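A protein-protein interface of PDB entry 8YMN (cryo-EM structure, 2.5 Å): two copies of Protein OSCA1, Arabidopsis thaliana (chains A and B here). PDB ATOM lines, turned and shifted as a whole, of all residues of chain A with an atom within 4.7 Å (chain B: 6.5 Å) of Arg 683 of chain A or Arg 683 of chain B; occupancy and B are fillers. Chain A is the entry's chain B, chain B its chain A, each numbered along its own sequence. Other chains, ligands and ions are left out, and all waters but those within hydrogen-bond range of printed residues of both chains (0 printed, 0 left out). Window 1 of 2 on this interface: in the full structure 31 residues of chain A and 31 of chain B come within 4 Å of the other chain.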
ATOM      1  N   GLN A 339      25.794   1.898   2.525  1.00  0.00           N
ATOM      2  CA  GLN A 339      26.522   2.798   3.402  1.00  0.00           C
ATOM      3  C   GLN A 339      25.649   3.844   4.078  1.00  0.00           C
ATOM      4  O   GLN A 339      26.116   4.931   4.397  1.00  0.00           O
ATOM      5  CB  GLN A 339      27.736   3.414   2.693  1.00  0.00           C
ATOM      6  CG  GLN A 339      27.482   4.266   1.468  1.00  0.00           C
ATOM      7  CD  GLN A 339      28.617   4.156   0.469  1.00  0.00           C
ATOM      8  OE1 GLN A 339      28.874   3.086  -0.076  1.00  0.00           O
ATOM      9  NE2 GLN A 339      29.308   5.260   0.234  1.00  0.00           N
ATOM     10  N   THR A 340      24.394   3.501   4.333  1.00  0.00           N
ATOM     11  CA  THR A 340      23.471   4.429   4.975  1.00  0.00           C
ATOM     12  C   THR A 340      22.675   3.733   6.071  1.00  0.00           C
ATOM     13  O   THR A 340      22.403   2.538   5.977  1.00  0.00           O
ATOM     14  CB  THR A 340      22.562   5.110   3.922  1.00  0.00           C
ATOM     15  OG1 THR A 340      22.760   6.528   3.955  1.00  0.00           O
ATOM     16  CG2 THR A 340      21.093   4.796   4.123  1.00  0.00           C
ATOM     17  N   THR A 341      22.348   4.451   7.142  1.00  0.00           N
ATOM     18  CA  THR A 341      21.513   3.878   8.194  1.00  0.00           C
ATOM     19  C   THR A 341      20.077   4.028   7.756  1.00  0.00           C
ATOM     20  O   THR A 341      19.681   5.079   7.266  1.00  0.00           O
ATOM     21  CB  THR A 341      21.745   4.533   9.567  1.00  0.00           C
ATOM     22  OG1 THR A 341      20.591   4.338  10.393  1.00  0.00           O
ATOM     23  CG2 THR A 341      22.018   6.018   9.419  1.00  0.00           C
ATOM     24  N   PRO A 679      39.094   2.831   3.085  1.00  0.00           N
ATOM     25  CA  PRO A 679      37.708   2.955   2.624  1.00  0.00           C
ATOM     26  C   PRO A 679      37.423   2.385   1.230  1.00  0.00           C
ATOM     27  O   PRO A 679      36.299   1.960   0.994  1.00  0.00           O
ATOM     28  CB  PRO A 679      37.465   4.471   2.650  1.00  0.00           C
ATOM     29  CG  PRO A 679      38.805   5.103   2.835  1.00  0.00           C
ATOM     30  CD  PRO A 679      39.580   4.110   3.628  1.00  0.00           C
ATOM     31  N   ALA A 680      38.406   2.365   0.336  1.00  0.00           N
ATOM     32  CA  ALA A 680      38.230   1.801  -0.999  1.00  0.00           C
ATOM     33  C   ALA A 680      37.873   0.331  -0.969  1.00  0.00           C
ATOM     34  O   ALA A 680      37.239  -0.170  -1.890  1.00  0.00           O
ATOM     35  CB  ALA A 680      39.496   2.000  -1.812  1.00  0.00           C
ATOM     36  N   PHE A 681      38.265  -0.363   0.088  1.00  0.00           N
ATOM     37  CA  PHE A 681      38.034  -1.791   0.174  1.00  0.00           C
ATOM     38  C   PHE A 681      36.737  -2.142   0.871  1.00  0.00           C
ATOM     39  O   PHE A 681      36.300  -3.288   0.824  1.00  0.00           O
ATOM     40  CB  PHE A 681      39.199  -2.448   0.902  1.00  0.00           C
ATOM     41  CG  PHE A 681      40.519  -2.274   0.217  1.00  0.00           C
ATOM     42  CD1 PHE A 681      41.321  -1.183   0.491  1.00  0.00           C
ATOM     43  CD2 PHE A 681      40.965  -3.210  -0.691  1.00  0.00           C
ATOM     44  CE1 PHE A 681      42.534  -1.023  -0.140  1.00  0.00           C
ATOM     45  CE2 PHE A 681      42.177  -3.059  -1.325  1.00  0.00           C
ATOM     46  CZ  PHE A 681      42.966  -1.967  -1.045  1.00  0.00           C
ATOM     47  N   VAL A 682      36.111  -1.166   1.512  1.00  0.00           N
ATOM     48  CA  VAL A 682      34.901  -1.444   2.272  1.00  0.00           C
ATOM     49  C   VAL A 682      33.655  -0.777   1.702  1.00  0.00           C
ATOM     50  O   VAL A 682      32.566  -1.339   1.775  1.00  0.00           O
ATOM     51  CB  VAL A 682      35.072  -1.061   3.755  1.00  0.00           C
ATOM     52  CG1 VAL A 682      35.827  -2.150   4.499  1.00  0.00           C
ATOM     53  CG2 VAL A 682      35.784   0.274   3.891  1.00  0.00           C
ATOM     54  N   ARG A 683      33.808   0.414   1.133  1.00  0.00           N
ATOM     55  CA  ARG A 683      32.668   1.136   0.579  1.00  0.00           C
ATOM     56  C   ARG A 683      32.890   1.466  -0.874  1.00  0.00           C
ATOM     57  O   ARG A 683      33.980   1.876  -1.246  1.00  0.00           O
ATOM     58  CB  ARG A 683      32.429   2.432   1.351  1.00  0.00           C
ATOM     59  CG  ARG A 683      31.819   2.243   2.726  1.00  0.00           C
ATOM     60  CD  ARG A 683      32.235   3.365   3.658  1.00  0.00           C
ATOM     61  NE  ARG A 683      31.094   3.926   4.374  1.00  0.00           N
ATOM     62  CZ  ARG A 683      30.582   5.129   4.137  1.00  0.00           C
ATOM     63  NH1 ARG A 683      31.109   5.902   3.201  1.00  0.00           N
ATOM     64  NH2 ARG A 683      29.543   5.558   4.837  1.00  0.00           N
ATOM     65  N   TYR A 684      31.868   1.285  -1.699  1.00  0.00           N
ATOM     66  CA  TYR A 684      31.969   1.648  -3.101  1.00  0.00           C
ATOM     67  C   TYR A 684      31.709   3.137  -3.201  1.00  0.00           C
ATOM     68  O   TYR A 684      30.630   3.602  -2.845  1.00  0.00           O
ATOM     69  CB  TYR A 684      30.933   0.882  -3.925  1.00  0.00           C
ATOM     70  CG  TYR A 684      31.226   0.785  -5.405  1.00  0.00           C
ATOM     71  CD1 TYR A 684      32.501   1.008  -5.900  1.00  0.00           C
ATOM     72  CD2 TYR A 684      30.226   0.459  -6.306  1.00  0.00           C
ATOM     73  CE1 TYR A 684      32.769   0.919  -7.251  1.00  0.00           C
ATOM     74  CE2 TYR A 684      30.485   0.362  -7.659  1.00  0.00           C
ATOM     75  CZ  TYR A 684      31.758   0.597  -8.126  1.00  0.00           C
ATOM     76  OH  TYR A 684      32.026   0.507  -9.470  1.00  0.00           O
ATOM     77  N   PRO A 685      32.702   3.901  -3.679  1.00  0.00           N
ATOM     78  CA  PRO A 685      32.458   5.329  -3.870  1.00  0.00           C
ATOM     79  C   PRO A 685      31.280   5.576  -4.795  1.00  0.00           C
ATOM     80  O   PRO A 685      31.117   4.862  -5.776  1.00  0.00           O
ATOM     81  CB  PRO A 685      33.763   5.838  -4.484  1.00  0.00           C
ATOM     82  CG  PRO A 685      34.554   4.632  -4.858  1.00  0.00           C
ATOM     83  CD  PRO A 685      34.094   3.529  -3.970  1.00  0.00           C
ATOM     84  N   ARG B 188      15.822  12.956  21.071  1.00  0.00           N
ATOM     85  CA  ARG B 188      16.471  13.587  19.933  1.00  0.00           C
ATOM     86  C   ARG B 188      15.724  13.280  18.660  1.00  0.00           C
ATOM     87  O   ARG B 188      15.545  14.150  17.822  1.00  0.00           O
ATOM     88  CB  ARG B 188      17.928  13.131  19.836  1.00  0.00           C
ATOM     89  CG  ARG B 188      18.449  12.904  18.431  1.00  0.00           C
ATOM     90  CD  ARG B 188      19.959  12.973  18.399  1.00  0.00           C
ATOM     91  NE  ARG B 188      20.467  13.182  17.051  1.00  0.00           N
ATOM     92  CZ  ARG B 188      21.188  14.232  16.682  1.00  0.00           C
ATOM     93  NH1 ARG B 188      21.485  15.170  17.564  1.00  0.00           N
ATOM     94  NH2 ARG B 188      21.612  14.343  15.433  1.00  0.00           N
ATOM     95  N   LEU B 189      15.256  12.048  18.522  1.00  0.00           N
ATOM     96  CA  LEU B 189      14.556  11.650  17.320  1.00  0.00           C
ATOM     97  C   LEU B 189      13.187  12.291  17.261  1.00  0.00           C
ATOM     98  O   LEU B 189      12.743  12.690  16.190  1.00  0.00           O
ATOM     99  CB  LEU B 189      14.469  10.131  17.249  1.00  0.00           C
ATOM    100  CG  LEU B 189      15.773   9.432  16.865  1.00  0.00           C
ATOM    101  CD1 LEU B 189      15.701   7.948  17.178  1.00  0.00           C
ATOM    102  CD2 LEU B 189      16.099   9.665  15.400  1.00  0.00           C
ATOM    103  N   ALA B 338      25.567  12.825   3.316  1.00  0.00           N
ATOM    104  CA  ALA B 338      26.351  12.921   4.532  1.00  0.00           C
ATOM    105  C   ALA B 338      26.933  11.592   4.967  1.00  0.00           C
ATOM    106  O   ALA B 338      28.032  11.548   5.508  1.00  0.00           O
ATOM    107  CB  ALA B 338      25.511  13.503   5.643  1.00  0.00           C
ATOM    108  N   GLN B 339      26.202  10.505   4.748  1.00  0.00           N
ATOM    109  CA  GLN B 339      26.672   9.207   5.195  1.00  0.00           C
ATOM    110  C   GLN B 339      27.140   8.296   4.071  1.00  0.00           C
ATOM    111  O   GLN B 339      27.065   7.078   4.186  1.00  0.00           O
ATOM    112  CB  GLN B 339      25.651   8.527   6.117  1.00  0.00           C
ATOM    113  CG  GLN B 339      24.284   8.215   5.549  1.00  0.00           C
ATOM    114  CD  GLN B 339      23.205   8.306   6.611  1.00  0.00           C
ATOM    115  OE1 GLN B 339      22.957   9.373   7.166  1.00  0.00           O
ATOM    116  NE2 GLN B 339      22.569   7.184   6.906  1.00  0.00           N
ATOM    117  N   THR B 340      27.659   8.884   3.002  1.00  0.00           N
ATOM    118  CA  THR B 340      28.135   8.105   1.866  1.00  0.00           C
ATOM    119  C   THR B 340      29.487   8.616   1.384  1.00  0.00           C
ATOM    120  O   THR B 340      29.778   9.805   1.499  1.00  0.00           O
ATOM    121  CB  THR B 340      27.073   8.080   0.739  1.00  0.00           C
ATOM    122  OG1 THR B 340      26.671   6.730   0.480  1.00  0.00           O
ATOM    123  CG2 THR B 340      27.564   8.720  -0.545  1.00  0.00           C
ATOM    124  N   THR B 341      30.343   7.721   0.899  1.00  0.00           N
ATOM    125  CA  THR B 341      31.623   8.146   0.340  1.00  0.00           C
ATOM    126  C   THR B 341      31.371   8.559  -1.090  1.00  0.00           C
ATOM    127  O   THR B 341      30.664   7.875  -1.821  1.00  0.00           O
ATOM    128  CB  THR B 341      32.704   7.054   0.419  1.00  0.00           C
ATOM    129  OG1 THR B 341      33.708   7.299  -0.574  1.00  0.00           O
ATOM    130  CG2 THR B 341      32.101   5.679   0.202  1.00  0.00           C
ATOM    131  N   GLN B 342      31.938   9.678  -1.503  1.00  0.00           N
ATOM    132  CA  GLN B 342      31.646  10.196  -2.827  1.00  0.00           C
ATOM    133  C   GLN B 342      32.654   9.847  -3.892  1.00  0.00           C
ATOM    134  O   GLN B 342      32.291   9.697  -5.053  1.00  0.00           O
ATOM    135  CB  GLN B 342      31.518  11.714  -2.742  1.00  0.00           C
ATOM    136  CG  GLN B 342      30.795  12.206  -1.506  1.00  0.00           C
ATOM    137  CD  GLN B 342      29.296  12.115  -1.649  1.00  0.00           C
ATOM    138  OE1 GLN B 342      28.759  12.257  -2.743  1.00  0.00           O
ATOM    139  NE2 GLN B 342      28.613  11.877  -0.543  1.00  0.00           N
ATOM    140  N   TRP B 353      26.996  16.262   7.532  1.00  0.00           N
ATOM    141  CA  TRP B 353      25.810  17.051   7.824  1.00  0.00           C
ATOM    142  C   TRP B 353      26.239  18.444   8.216  1.00  0.00           C
ATOM    143  O   TRP B 353      27.084  18.613   9.090  1.00  0.00           O
ATOM    144  CB  TRP B 353      25.050  16.446   8.995  1.00  0.00           C
ATOM    145  CG  TRP B 353      23.980  15.474   8.643  1.00  0.00           C
ATOM    146  CD1 TRP B 353      23.928  14.155   8.986  1.00  0.00           C
ATOM    147  CD2 TRP B 353      22.784  15.745   7.908  1.00  0.00           C
ATOM    148  NE1 TRP B 353      22.780  13.583   8.496  1.00  0.00           N
ATOM    149  CE2 TRP B 353      22.060  14.542   7.832  1.00  0.00           C
ATOM    150  CE3 TRP B 353      22.258  16.886   7.303  1.00  0.00           C
ATOM    151  CZ2 TRP B 353      20.839  14.452   7.183  1.00  0.00           C
ATOM    152  CZ3 TRP B 353      21.052  16.789   6.655  1.00  0.00           C
ATOM    153  CH2 TRP B 353      20.354  15.583   6.599  1.00  0.00           C
ATOM    154  N   GLU B 678      24.309   5.293  20.006  1.00  0.00           N
ATOM    155  CA  GLU B 678      25.163   6.314  19.410  1.00  0.00           C
ATOM    156  C   GLU B 678      24.847   6.677  17.957  1.00  0.00           C
ATOM    157  O   GLU B 678      24.861   7.854  17.618  1.00  0.00           O
ATOM    158  CB  GLU B 678      26.638   5.948  19.562  1.00  0.00           C
ATOM    159  CG  GLU B 678      27.609   6.989  19.038  1.00  0.00           C
ATOM    160  CD  GLU B 678      28.947   6.932  19.738  1.00  0.00           C
ATOM    161  OE1 GLU B 678      28.965   6.687  20.963  1.00  0.00           O
ATOM    162  OE2 GLU B 678      29.978   7.131  19.066  1.00  0.00           O
ATOM    163  N   PRO B 679      24.561   5.689  17.084  1.00  0.00           N
ATOM    164  CA  PRO B 679      24.288   6.118  15.709  1.00  0.00           C
ATOM    165  C   PRO B 679      23.170   7.155  15.552  1.00  0.00           C
ATOM    166  O   PRO B 679      23.228   7.935  14.609  1.00  0.00           O
ATOM    167  CB  PRO B 679      23.914   4.807  15.001  1.00  0.00           C
ATOM    168  CG  PRO B 679      23.716   3.794  16.081  1.00  0.00           C
ATOM    169  CD  PRO B 679      24.640   4.222  17.167  1.00  0.00           C
ATOM    170  N   ALA B 680      22.188   7.175  16.446  1.00  0.00           N
ATOM    171  CA  ALA B 680      21.109   8.157  16.393  1.00  0.00           C
ATOM    172  C   ALA B 680      21.608   9.580  16.521  1.00  0.00           C
ATOM    173  O   ALA B 680      20.969  10.505  16.033  1.00  0.00           O
ATOM    174  CB  ALA B 680      20.100   7.872  17.491  1.00  0.00           C
ATOM    175  N   PHE B 681      22.751   9.762  17.162  1.00  0.00           N
ATOM    176  CA  PHE B 681      23.273  11.094  17.397  1.00  0.00           C
ATOM    177  C   PHE B 681      24.219  11.561  16.313  1.00  0.00           C
ATOM    178  O   PHE B 681      24.565  12.738  16.258  1.00  0.00           O
ATOM    179  CB  PHE B 681      23.983  11.126  18.744  1.00  0.00           C
ATOM    180  CG  PHE B 681      23.095  10.808  19.908  1.00  0.00           C
ATOM    181  CD1 PHE B 681      22.929   9.505  20.336  1.00  0.00           C
ATOM    182  CD2 PHE B 681      22.438  11.814  20.581  1.00  0.00           C
ATOM    183  CE1 PHE B 681      22.112   9.213  21.405  1.00  0.00           C
ATOM    184  CE2 PHE B 681      21.621  11.532  21.652  1.00  0.00           C
ATOM    185  CZ  PHE B 681      21.461  10.229  22.068  1.00  0.00           C
ATOM    186  N   VAL B 682      24.639  10.654  15.442  1.00  0.00           N
ATOM    187  CA  VAL B 682      25.611  11.011  14.421  1.00  0.00           C
ATOM    188  C   VAL B 682      25.059  10.943  13.002  1.00  0.00           C
ATOM    189  O   VAL B 682      25.445  11.739  12.151  1.00  0.00           O
ATOM    190  CB  VAL B 682      26.882  10.147  14.534  1.00  0.00           C
ATOM    191  CG1 VAL B 682      27.790  10.682  15.628  1.00  0.00           C
ATOM    192  CG2 VAL B 682      26.528   8.693  14.793  1.00  0.00           C
ATOM    193  N   ARG B 683      24.159  10.001  12.743  1.00  0.00           N
ATOM    194  CA  ARG B 683      23.591   9.848  11.408  1.00  0.00           C
ATOM    195  C   ARG B 683      22.088   9.945  11.444  1.00  0.00           C
ATOM    196  O   ARG B 683      21.462   9.380  12.330  1.00  0.00           O
ATOM    197  CB  ARG B 683      23.987   8.500  10.810  1.00  0.00           C
ATOM    198  CG  ARG B 683      25.431   8.411  10.357  1.00  0.00           C
ATOM    199  CD  ARG B 683      25.934   6.982  10.443  1.00  0.00           C
ATOM    200  NE  ARG B 683      26.616   6.574   9.219  1.00  0.00           N
ATOM    201  CZ  ARG B 683      26.122   5.707   8.343  1.00  0.00           C
ATOM    202  NH1 ARG B 683      24.939   5.152   8.553  1.00  0.00           N
ATOM    203  NH2 ARG B 683      26.812   5.394   7.257  1.00  0.00           N
ATOM    204  N   TYR B 684      21.504  10.660  10.493  1.00  0.00           N
ATOM    205  CA  TYR B 684      20.057  10.746  10.407  1.00  0.00           C
ATOM    206  C   TYR B 684      19.575   9.504   9.686  1.00  0.00           C
ATOM    207  O   TYR B 684      19.934   9.279   8.534  1.00  0.00           O
ATOM    208  CB  TYR B 684      19.644  11.995   9.627  1.00  0.00           C
ATOM    209  CG  TYR B 684      18.227  12.466   9.864  1.00  0.00           C
ATOM    210  CD1 TYR B 684      17.511  12.057  10.977  1.00  0.00           C
ATOM    211  CD2 TYR B 684      17.609  13.331   8.975  1.00  0.00           C
ATOM    212  CE1 TYR B 684      16.219  12.487  11.194  1.00  0.00           C
ATOM    213  CE2 TYR B 684      16.318  13.772   9.186  1.00  0.00           C
ATOM    214  CZ  TYR B 684      15.626  13.343  10.296  1.00  0.00           C
ATOM    215  OH  TYR B 684      14.340  13.773  10.513  1.00  0.00           O
ATOM    216  N   PRO B 685      18.762   8.680  10.362  1.00  0.00           N
ATOM    217  CA  PRO B 685      18.208   7.517   9.671  1.00  0.00           C
ATOM    218  C   PRO B 685      17.430   7.922   8.432  1.00  0.00           C
ATOM    219  O   PRO B 685      16.727   8.925   8.456  1.00  0.00           O
ATOM    220  CB  PRO B 685      17.294   6.879  10.717  1.00  0.00           C
ATOM    221  CG  PRO B 685      17.170   7.862  11.829  1.00  0.00           C
ATOM    222  CD  PRO B 685      18.393   8.712  11.785  1.00  0.00           C
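Among the printed residues, merely in contact across the chains: Thr 340 of chain A with Arg 683 of chain B, Thr 341 of chain A with Tyr 684 of chain B, Thr 341 of chain A with Pro 685 of chain B, Arg 683 of chain A with Thr 340 of chain B, Arg 683 of chain A with Arg 683 of chain B, Tyr 684 of chain A with Thr 341 of chain B and Pro 685 of chain A with Thr 341 of chain B.
Arg 683 of chain A touches four residues of chain B.
Of the printed residues of chain B, Pro 685 of chain A touches Thr 341.
Gln 342 of chain B touches none of the printed residues of chain A.
Arg 683 of chain B touches just these residues of chain A: Gln 339 (3.0 Å), Thr 340 (3.6 Å), Thr 341 (3.0 Å) and Arg 683 (3.7 Å).
Of the printed residues of chain A, Pro 685 of chain B touches Thr 341 (3.7 Å).
Along chain B the printed residues that touch a printed residue of chain A span positions 339 to 685.
Among the printed residues, no Asp or Glu carboxylate lies within 4 Å of a Lys or Arg side-chain nitrogen of the other chain.
The side-chain amide oxygen (OE1) of Gln 339 of chain B sits close to the backbone carbonyl oxygen (O) of Tyr 684 of chain B (3.3 Å).
The backbone carbonyl oxygen (O) of Thr 340 of chain B sits at hydrogen-bond distance from the side-chain amide nitrogen (NE2) of Gln 342 of chain B (3.1 Å).
OE1 of Gln 339 of chain A sits close to O of Tyr 684 of chain A (3.3 Å).
The side-chain amide nitrogen of Gln 339 of chain B lies close to the side-chain hydroxyl of Thr 340 of chain A (3.0 Å).
N of Thr 341 of chain A sits close to NE2 of Gln 339 of chain B.
The guanidinium group of Arg 683 of chain A sits at hydrogen-bond distance from the backbone carbonyl oxygen of Gln 339 of chain B (3.0 Å).
OG1 of Thr 340 of chain B lies close to NE2 of Gln 339 of chain A (3.0 Å).
NE2 of Gln 339 of chain A lies close to N of Thr 341 of chain B (2.8 Å).
The backbone carbonyl oxygen of Gln 339 of chain A sits at hydrogen-bond distance from the guanidinium group of Arg 683 of chain B.
O of Gln 339 of chain A lies close to O of Gln 339 of chain B (2.4 Å).
The backbone NH (N) of Thr 341 of chain A sits close to the guanidinium group (NH1) of Arg 683 of chain B, at 3.0 Å.
The backbone NH (N) of Thr 341 of chain B sits close to the guanidinium group (NH1) of Arg 683 of chain A, 3.0 Å away.
Gln 339 of chain B touches its own counterpart, Gln 339 of chain A.
Gln 339 of chain A touches Arg 683 of chain B, and with the chains exchanged Arg 683 of chain A touches Gln 339 of chain B.
Thr 340 of chain A touches Arg 683 of chain B, and with the chains exchanged Arg 683 of chain A touches Thr 340 of chain B.
Thr 341 of chain A touches Tyr 684 of chain B, and with the chains exchanged Tyr 684 of chain A touches Thr 341 of chain B.
Positions printed for both chains: 339, 340, 341, 679, 680, 681, 682, 683, 684 and 685.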
